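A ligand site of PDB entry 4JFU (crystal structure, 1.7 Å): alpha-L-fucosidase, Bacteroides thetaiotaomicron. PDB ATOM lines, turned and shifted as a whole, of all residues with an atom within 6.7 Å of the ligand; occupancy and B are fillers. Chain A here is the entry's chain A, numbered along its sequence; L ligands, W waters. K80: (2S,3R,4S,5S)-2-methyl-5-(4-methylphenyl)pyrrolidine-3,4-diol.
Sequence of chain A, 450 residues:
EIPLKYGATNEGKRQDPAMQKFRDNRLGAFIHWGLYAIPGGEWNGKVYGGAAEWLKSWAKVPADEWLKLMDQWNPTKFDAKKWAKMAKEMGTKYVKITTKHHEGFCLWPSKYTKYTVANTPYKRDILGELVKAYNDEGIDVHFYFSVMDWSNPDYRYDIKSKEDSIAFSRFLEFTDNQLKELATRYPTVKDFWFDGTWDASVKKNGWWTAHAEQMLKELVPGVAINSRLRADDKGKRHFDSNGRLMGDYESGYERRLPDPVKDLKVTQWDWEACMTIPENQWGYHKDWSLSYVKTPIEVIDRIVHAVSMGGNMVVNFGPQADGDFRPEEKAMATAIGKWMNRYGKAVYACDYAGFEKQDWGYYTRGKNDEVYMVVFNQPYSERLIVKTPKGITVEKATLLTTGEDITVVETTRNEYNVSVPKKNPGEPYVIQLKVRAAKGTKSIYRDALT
OAH of the ligand sits at hydrogen-bond distance from NE2 of His 101 (2.8 Å).
A ring nitrogen (NE2) of His 32 lies within hydrogen-bond range of an oxygen (OAH) of the ligand, 2.7 Å away.
The side-chain carboxylate of Asp 195 lies within salt-bridge range of a nitrogen (NAD) of the ligand, at 2.8 Å.
The side-chain carboxylate (OE1) of Glu 254 is in salt-bridge range of a nitrogen (NAD) of the ligand, 3.3 Å away.
The indole nitrogen (NE1) of Trp 54 is in hydrogen-bond range of an oxygen (OAG) of the ligand (3.2 Å).
The side-chain carboxylate of Glu 53 sits at hydrogen-bond distance from an oxygen (OAG) of the ligand (2.7 Å).
A ring nitrogen (NE2) of His 101 lies close to the side-chain hydroxyl (OH) of Tyr 144 (3.1 Å).
The side-chain carboxylate (OE1) of Glu 53 lies within hydrogen-bond range of the backbone NH (N) of Trp 282, at 3.2 Å.
The side-chain carboxylate (OE2) of Glu 254 lies within salt-bridge range of the guanidinium group (NH1) of Arg 228 (3.0 Å).
The side-chain carboxylate of Asp 195 sits at hydrogen-bond distance from the side-chain hydroxyl of Tyr 144 (2.7 Å).
NE2 of His 102 lies close to NE1 of Trp 54, 3.4 Å away.
The backbone NH (N) of Gly 283 is in hydrogen-bond range of the side-chain carboxylate (OE1) of Glu 53.
Residues that only touch the ligand: Tyr 144, Trp 282, Trp 198, His 102 and Trp 193.
11 residues have an atom within 4 Å of the ligand: His 32, Glu 53, Trp 54, His 101, His 102, Tyr 144, Trp 193, Asp 195, Trp 198, Glu 254 and Trp 282.
The nearest printed residue that does not touch the ligand is Cys 274 (4.8 Å).
Water W1 lies within hydrogen-bond range of the side-chain carboxylate (OD1) of Asp 195 (2.6 Å), the side-chain carboxylate (OE2) of Glu 254 (3.0 Å) and a nitrogen (NAD) of the ligand (3.0 Å).
Water W2 lies within hydrogen-bond range of the side-chain carboxylate (OE1) of Glu 254, the guanidinium group (NE) of Arg 255 and the indole nitrogen (NE1) of Trp 282.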
ATOM      1  N   PHE A  30      12.612  22.272 -28.511  1.00  0.00           N
ATOM      2  CA  PHE A  30      13.463  21.650 -27.496  1.00  0.00           C
ATOM      3  C   PHE A  30      14.524  20.860 -28.267  1.00  0.00           C
ATOM      4  O   PHE A  30      14.207  20.248 -29.329  1.00  0.00           O
ATOM      5  CB  PHE A  30      12.644  20.629 -26.686  1.00  0.00           C
ATOM      6  CG  PHE A  30      12.887  20.701 -25.192  1.00  0.00           C
ATOM      7  CD1 PHE A  30      14.152  20.457 -24.677  1.00  0.00           C
ATOM      8  CD2 PHE A  30      11.831  20.999 -24.326  1.00  0.00           C
ATOM      9  CE1 PHE A  30      14.389  20.524 -23.309  1.00  0.00           C
ATOM     10  CE2 PHE A  30      12.076  21.070 -22.935  1.00  0.00           C
ATOM     11  CZ  PHE A  30      13.342  20.825 -22.442  1.00  0.00           C
ATOM     12  N   HIS A  32      17.018  17.671 -27.420  1.00  0.00           N
ATOM     13  CA  HIS A  32      17.622  16.654 -26.535  1.00  0.00           C
ATOM     14  C   HIS A  32      18.743  16.017 -27.297  1.00  0.00           C
ATOM     15  O   HIS A  32      18.504  15.314 -28.307  1.00  0.00           O
ATOM     16  CB  HIS A  32      16.599  15.552 -26.168  1.00  0.00           C
ATOM     17  CG  HIS A  32      15.764  15.883 -24.967  1.00  0.00           C
ATOM     18  ND1 HIS A  32      14.752  16.830 -25.000  1.00  0.00           N
ATOM     19  CD2 HIS A  32      15.783  15.382 -23.709  1.00  0.00           C
ATOM     20  CE1 HIS A  32      14.206  16.914 -23.784  1.00  0.00           C
ATOM     21  NE2 HIS A  32      14.830  16.056 -22.983  1.00  0.00           N
ATOM     22  N   ALA A  51      12.055   5.351 -23.838  1.00  0.00           N
ATOM     23  CA  ALA A  51      12.660   6.584 -24.376  1.00  0.00           C
ATOM     24  C   ALA A  51      14.173   6.408 -24.544  1.00  0.00           C
ATOM     25  O   ALA A  51      14.862   5.959 -23.608  1.00  0.00           O
ATOM     26  CB  ALA A  51      12.389   7.722 -23.385  1.00  0.00           C
ATOM     27  N   GLU A  53      16.695   8.379 -24.522  1.00  0.00           N
ATOM     28  CA  GLU A  53      17.610   9.057 -23.605  1.00  0.00           C
ATOM     29  C   GLU A  53      17.750   8.348 -22.269  1.00  0.00           C
ATOM     30  O   GLU A  53      18.652   8.654 -21.509  1.00  0.00           O
ATOM     31  CB  GLU A  53      17.267  10.553 -23.445  1.00  0.00           C
ATOM     32  CG  GLU A  53      15.999  10.833 -22.654  1.00  0.00           C
ATOM     33  CD  GLU A  53      14.682  10.552 -23.342  1.00  0.00           C
ATOM     34  OE1 GLU A  53      14.639  10.159 -24.543  1.00  0.00           O
ATOM     35  OE2 GLU A  53      13.662  10.665 -22.622  1.00  0.00           O
ATOM     36  N   TRP A  54      16.855   7.385 -21.989  1.00  0.00           N
ATOM     37  CA  TRP A  54      16.909   6.517 -20.802  1.00  0.00           C
ATOM     38  C   TRP A  54      17.513   5.103 -21.085  1.00  0.00           C
ATOM     39  O   TRP A  54      17.433   4.222 -20.238  1.00  0.00           O
ATOM     40  CB  TRP A  54      15.458   6.337 -20.255  1.00  0.00           C
ATOM     41  CG  TRP A  54      15.014   7.466 -19.360  1.00  0.00           C
ATOM     42  CD1 TRP A  54      14.629   8.723 -19.724  1.00  0.00           C
ATOM     43  CD2 TRP A  54      14.918   7.384 -17.948  1.00  0.00           C
ATOM     44  NE1 TRP A  54      14.298   9.476 -18.568  1.00  0.00           N
ATOM     45  CE2 TRP A  54      14.495   8.661 -17.477  1.00  0.00           C
ATOM     46  CE3 TRP A  54      15.171   6.357 -17.019  1.00  0.00           C
ATOM     47  CZ2 TRP A  54      14.299   8.930 -16.113  1.00  0.00           C
ATOM     48  CZ3 TRP A  54      14.990   6.644 -15.651  1.00  0.00           C
ATOM     49  CH2 TRP A  54      14.555   7.929 -15.220  1.00  0.00           C
ATOM     50  N   THR A  98      19.148  20.684 -23.884  1.00  0.00           N
ATOM     51  CA  THR A  98      19.743  19.825 -22.810  1.00  0.00           C
ATOM     52  C   THR A  98      21.226  20.153 -22.601  1.00  0.00           C
ATOM     53  O   THR A  98      22.077  19.767 -23.399  1.00  0.00           O
ATOM     54  CB  THR A  98      19.641  18.302 -23.151  1.00  0.00           C
ATOM     55  OG1 THR A  98      20.196  18.085 -24.454  1.00  0.00           O
ATOM     56  CG2 THR A  98      18.194  17.864 -23.121  1.00  0.00           C
ATOM     57  N   HIS A 101      21.833  15.878 -19.558  1.00  0.00           N
ATOM     58  CA  HIS A 101      20.673  15.029 -19.204  1.00  0.00           C
ATOM     59  C   HIS A 101      21.008  14.092 -18.020  1.00  0.00           C
ATOM     60  O   HIS A 101      22.066  14.267 -17.390  1.00  0.00           O
ATOM     61  CB  HIS A 101      20.152  14.277 -20.447  1.00  0.00           C
ATOM     62  CG  HIS A 101      18.697  13.902 -20.348  1.00  0.00           C
ATOM     63  ND1 HIS A 101      18.274  12.691 -19.857  1.00  0.00           N
ATOM     64  CD2 HIS A 101      17.576  14.568 -20.721  1.00  0.00           C
ATOM     65  CE1 HIS A 101      16.945  12.643 -19.868  1.00  0.00           C
ATOM     66  NE2 HIS A 101      16.501  13.760 -20.420  1.00  0.00           N
ATOM     67  N   HIS A 102      20.155  13.091 -17.723  1.00  0.00           N
ATOM     68  CA  HIS A 102      20.408  12.256 -16.551  1.00  0.00           C
ATOM     69  C   HIS A 102      21.775  11.571 -16.643  1.00  0.00           C
ATOM     70  O   HIS A 102      22.454  11.366 -15.633  1.00  0.00           O
ATOM     71  CB  HIS A 102      19.291  11.201 -16.343  1.00  0.00           C
ATOM     72  CG  HIS A 102      17.882  11.727 -16.438  1.00  0.00           C
ATOM     73  ND1 HIS A 102      17.496  12.985 -15.995  1.00  0.00           N
ATOM     74  CD2 HIS A 102      16.755  11.127 -16.906  1.00  0.00           C
ATOM     75  CE1 HIS A 102      16.189  13.128 -16.198  1.00  0.00           C
ATOM     76  NE2 HIS A 102      15.722  12.019 -16.740  1.00  0.00           N
ATOM     77  N   TYR A 144      17.934  23.450 -20.388  1.00  0.00           N
ATOM     78  CA  TYR A 144      17.433  22.308 -19.627  1.00  0.00           C
ATOM     79  C   TYR A 144      18.626  21.816 -18.793  1.00  0.00           C
ATOM     80  O   TYR A 144      19.754  21.776 -19.279  1.00  0.00           O
ATOM     81  CB  TYR A 144      17.053  21.191 -20.645  1.00  0.00           C
ATOM     82  CG  TYR A 144      16.820  19.818 -20.031  1.00  0.00           C
ATOM     83  CD1 TYR A 144      17.902  19.056 -19.520  1.00  0.00           C
ATOM     84  CD2 TYR A 144      15.530  19.270 -19.957  1.00  0.00           C
ATOM     85  CE1 TYR A 144      17.710  17.762 -18.954  1.00  0.00           C
ATOM     86  CE2 TYR A 144      15.342  17.962 -19.417  1.00  0.00           C
ATOM     87  CZ  TYR A 144      16.416  17.263 -18.896  1.00  0.00           C
ATOM     88  OH  TYR A 144      16.286  16.006 -18.316  1.00  0.00           O
ATOM     89  N   MET A 148      19.304  15.155 -11.136  1.00  0.00           N
ATOM     90  CA  MET A 148      19.696  13.727 -11.104  1.00  0.00           C
ATOM     91  C   MET A 148      20.829  13.502 -12.123  1.00  0.00           C
ATOM     92  O   MET A 148      20.734  13.935 -13.300  1.00  0.00           O
ATOM     93  CB  MET A 148      18.505  12.830 -11.399  1.00  0.00           C
ATOM     94  CG  MET A 148      18.912  11.361 -11.504  1.00  0.00           C
ATOM     95  SD  MET A 148      17.459  10.308 -11.600  1.00  0.00           S
ATOM     96  CE  MET A 148      16.896  10.608 -13.286  1.00  0.00           C
ATOM     97  N   TRP A 193      15.423  25.319 -17.081  1.00  0.00           N
ATOM     98  CA  TRP A 193      14.329  24.380 -16.989  1.00  0.00           C
ATOM     99  C   TRP A 193      14.893  23.090 -16.343  1.00  0.00           C
ATOM    100  O   TRP A 193      15.622  22.283 -16.969  1.00  0.00           O
ATOM    101  CB  TRP A 193      13.784  24.120 -18.400  1.00  0.00           C
ATOM    102  CG  TRP A 193      12.421  23.436 -18.439  1.00  0.00           C
ATOM    103  CD1 TRP A 193      11.225  24.050 -18.544  1.00  0.00           C
ATOM    104  CD2 TRP A 193      12.157  22.006 -18.389  1.00  0.00           C
ATOM    105  NE1 TRP A 193      10.197  23.106 -18.552  1.00  0.00           N
ATOM    106  CE2 TRP A 193      10.747  21.848 -18.469  1.00  0.00           C
ATOM    107  CE3 TRP A 193      12.965  20.860 -18.296  1.00  0.00           C
ATOM    108  CZ2 TRP A 193      10.114  20.582 -18.495  1.00  0.00           C
ATOM    109  CZ3 TRP A 193      12.339  19.570 -18.307  1.00  0.00           C
ATOM    110  CH2 TRP A 193      10.915  19.456 -18.345  1.00  0.00           C
ATOM    111  N   ASP A 195      15.050  19.436 -14.540  1.00  0.00           N
ATOM    112  CA  ASP A 195      14.427  18.100 -14.549  1.00  0.00           C
ATOM    113  C   ASP A 195      15.105  17.214 -13.538  1.00  0.00           C
ATOM    114  O   ASP A 195      16.140  17.582 -12.994  1.00  0.00           O
ATOM    115  CB  ASP A 195      14.610  17.522 -15.965  1.00  0.00           C
ATOM    116  CG  ASP A 195      13.613  16.427 -16.301  1.00  0.00           C
ATOM    117  OD1 ASP A 195      12.647  16.171 -15.543  1.00  0.00           O
ATOM    118  OD2 ASP A 195      13.767  15.850 -17.400  1.00  0.00           O
ATOM    119  N   GLY A 196      14.601  15.987 -13.318  1.00  0.00           N
ATOM    120  CA  GLY A 196      15.354  15.068 -12.437  1.00  0.00           C
ATOM    121  C   GLY A 196      15.372  15.561 -10.995  1.00  0.00           C
ATOM    122  O   GLY A 196      16.373  15.424 -10.321  1.00  0.00           O
ATOM    123  N   TRP A 198      12.677  14.891  -8.793  1.00  0.00           N
ATOM    124  CA  TRP A 198      11.548  14.234  -8.112  1.00  0.00           C
ATOM    125  C   TRP A 198      12.009  13.293  -6.972  1.00  0.00           C
ATOM    126  O   TRP A 198      11.163  12.772  -6.254  1.00  0.00           O
ATOM    127  CB  TRP A 198      10.701  13.399  -9.104  1.00  0.00           C
ATOM    128  CG  TRP A 198      11.548  12.442  -9.834  1.00  0.00           C
ATOM    129  CD1 TRP A 198      12.069  11.284  -9.349  1.00  0.00           C
ATOM    130  CD2 TRP A 198      12.059  12.593 -11.161  1.00  0.00           C
ATOM    131  NE1 TRP A 198      12.841  10.680 -10.297  1.00  0.00           N
ATOM    132  CE2 TRP A 198      12.864  11.453 -11.418  1.00  0.00           C
ATOM    133  CE3 TRP A 198      11.887  13.565 -12.161  1.00  0.00           C
ATOM    134  CZ2 TRP A 198      13.517  11.250 -12.641  1.00  0.00           C
ATOM    135  CZ3 TRP A 198      12.535  13.345 -13.411  1.00  0.00           C
ATOM    136  CH2 TRP A 198      13.341  12.198 -13.618  1.00  0.00           C
ATOM    137  N   ARG A 228       9.252  22.907 -11.948  1.00  0.00           N
ATOM    138  CA  ARG A 228       9.656  21.557 -11.669  1.00  0.00           C
ATOM    139  C   ARG A 228      10.897  21.507 -10.779  1.00  0.00           C
ATOM    140  O   ARG A 228      11.153  20.492 -10.132  1.00  0.00           O
ATOM    141  CB  ARG A 228       9.876  20.808 -13.008  1.00  0.00           C
ATOM    142  CG  ARG A 228      10.353  19.363 -12.883  1.00  0.00           C
ATOM    143  CD  ARG A 228      10.270  18.693 -14.251  1.00  0.00           C
ATOM    144  NE  ARG A 228       8.878  18.300 -14.431  1.00  0.00           N
ATOM    145  CZ  ARG A 228       8.124  18.380 -15.536  1.00  0.00           C
ATOM    146  NH1 ARG A 228       8.573  18.870 -16.667  1.00  0.00           N
ATOM    147  NH2 ARG A 228       6.866  17.970 -15.485  1.00  0.00           N
ATOM    148  N   GLU A 254       3.545  17.896 -19.943  1.00  0.00           N
ATOM    149  CA  GLU A 254       4.637  17.318 -20.673  1.00  0.00           C
ATOM    150  C   GLU A 254       3.954  16.176 -21.353  1.00  0.00           C
ATOM    151  O   GLU A 254       3.499  15.208 -20.701  1.00  0.00           O
ATOM    152  CB  GLU A 254       5.741  16.870 -19.684  1.00  0.00           C
ATOM    153  CG  GLU A 254       6.874  16.068 -20.308  1.00  0.00           C
ATOM    154  CD  GLU A 254       8.011  15.689 -19.339  1.00  0.00           C
ATOM    155  OE1 GLU A 254       8.488  14.550 -19.403  1.00  0.00           O
ATOM    156  OE2 GLU A 254       8.436  16.523 -18.516  1.00  0.00           O
ATOM    157  N   ARG A 255       3.766  16.332 -22.650  1.00  0.00           N
ATOM    158  CA  ARG A 255       3.106  15.341 -23.488  1.00  0.00           C
ATOM    159  C   ARG A 255       1.591  15.254 -23.118  1.00  0.00           C
ATOM    160  O   ARG A 255       0.916  14.261 -23.370  1.00  0.00           O
ATOM    161  CB  ARG A 255       3.831  13.978 -23.419  1.00  0.00           C
ATOM    162  CG  ARG A 255       5.334  14.009 -23.898  1.00  0.00           C
ATOM    163  CD  ARG A 255       5.953  12.600 -24.020  1.00  0.00           C
ATOM    164  NE  ARG A 255       5.746  11.872 -22.738  1.00  0.00           N
ATOM    165  CZ  ARG A 255       4.911  10.848 -22.506  1.00  0.00           C
ATOM    166  NH1 ARG A 255       4.195  10.317 -23.490  1.00  0.00           N
ATOM    167  NH2 ARG A 255       4.808  10.305 -21.282  1.00  0.00           N
ATOM    168  N   CYS A 274       5.599  21.047 -23.085  1.00  0.00           N
ATOM    169  CA  CYS A 274       6.616  20.566 -24.020  1.00  0.00           C
ATOM    170  C   CYS A 274       6.093  19.255 -24.555  1.00  0.00           C
ATOM    171  O   CYS A 274       5.258  18.593 -23.897  1.00  0.00           O
ATOM    172  CB  CYS A 274       7.960  20.360 -23.338  1.00  0.00           C
ATOM    173  SG  CYS A 274       7.856  19.328 -21.871  1.00  0.00           S
ATOM    174  N   ASN A 280       6.672   8.988 -27.121  1.00  0.00           N
ATOM    175  CA  ASN A 280       7.526   9.173 -25.958  1.00  0.00           C
ATOM    176  C   ASN A 280       8.982   8.886 -26.307  1.00  0.00           C
ATOM    177  O   ASN A 280       9.551   7.888 -25.854  1.00  0.00           O
ATOM    178  CB  ASN A 280       7.079   8.241 -24.828  1.00  0.00           C
ATOM    179  CG  ASN A 280       7.692   8.596 -23.490  1.00  0.00           C
ATOM    180  OD1 ASN A 280       8.373   9.609 -23.328  1.00  0.00           O
ATOM    181  ND2 ASN A 280       7.509   7.703 -22.517  1.00  0.00           N
ATOM    182  N   TRP A 282      12.466  11.448 -26.580  1.00  0.00           N
ATOM    183  CA  TRP A 282      13.005  12.820 -26.572  1.00  0.00           C
ATOM    184  C   TRP A 282      14.356  12.822 -27.271  1.00  0.00           C
ATOM    185  O   TRP A 282      14.574  13.592 -28.205  1.00  0.00           O
ATOM    186  CB  TRP A 282      13.129  13.344 -25.127  1.00  0.00           C
ATOM    187  CG  TRP A 282      11.817  13.425 -24.408  1.00  0.00           C
ATOM    188  CD1 TRP A 282      11.176  12.410 -23.730  1.00  0.00           C
ATOM    189  CD2 TRP A 282      10.984  14.597 -24.266  1.00  0.00           C
ATOM    190  NE1 TRP A 282       9.993  12.886 -23.169  1.00  0.00           N
ATOM    191  CE2 TRP A 282       9.861  14.236 -23.491  1.00  0.00           C
ATOM    192  CE3 TRP A 282      11.100  15.930 -24.730  1.00  0.00           C
ATOM    193  CZ2 TRP A 282       8.829  15.147 -23.173  1.00  0.00           C
ATOM    194  CZ3 TRP A 282      10.076  16.851 -24.439  1.00  0.00           C
ATOM    195  CH2 TRP A 282       8.959  16.469 -23.663  1.00  0.00           C
ATOM    196  N   GLY A 283      15.286  12.010 -26.773  1.00  0.00           N
ATOM    197  CA  GLY A 283      16.544  11.796 -27.509  1.00  0.00           C
ATOM    198  C   GLY A 283      16.317  11.004 -28.815  1.00  0.00           C
ATOM    199  O   GLY A 283      15.263  10.385 -29.029  1.00  0.00           O
HETATM  200  CAJ K80 L   1      11.965  11.779 -16.942  1.00  0.00           C
HETATM  201  CAK K80 L   1      11.175  10.882 -16.217  1.00  0.00           C
HETATM  202  CAL K80 L   1       9.906  10.555 -16.664  1.00  0.00           C
HETATM  203  CAO K80 L   1       9.132   9.637 -15.901  1.00  0.00           C
HETATM  204  CAM K80 L   1       9.404  11.103 -17.862  1.00  0.00           C
HETATM  205  CAN K80 L   1      10.213  12.005 -18.586  1.00  0.00           C
HETATM  206  CAI K80 L   1      11.488  12.344 -18.122  1.00  0.00           C
HETATM  207  CAC K80 L   1      12.360  13.280 -18.818  1.00  0.00           C
HETATM  208  NAD K80 L   1      11.742  14.634 -18.932  1.00  0.00           N
HETATM  209  CAE K80 L   1      11.541  14.954 -20.389  1.00  0.00           C
HETATM  210  CAF K80 L   1      11.545  16.446 -20.718  1.00  0.00           C
HETATM  211  CAA K80 L   1      12.723  14.235 -21.015  1.00  0.00           C
HETATM  212  OAH K80 L   1      13.985  14.887 -20.723  1.00  0.00           O
HETATM  213  CAB K80 L   1      12.613  12.862 -20.298  1.00  0.00           C
HETATM  214  OAG K80 L   1      13.827  12.093 -20.382  1.00  0.00           O
HETATM  215  O   HOH W   1      10.270  15.393 -16.397  1.00  0.00           O
HETATM  216  O   HOH W   2       7.708  12.511 -20.799  1.00  0.00           O
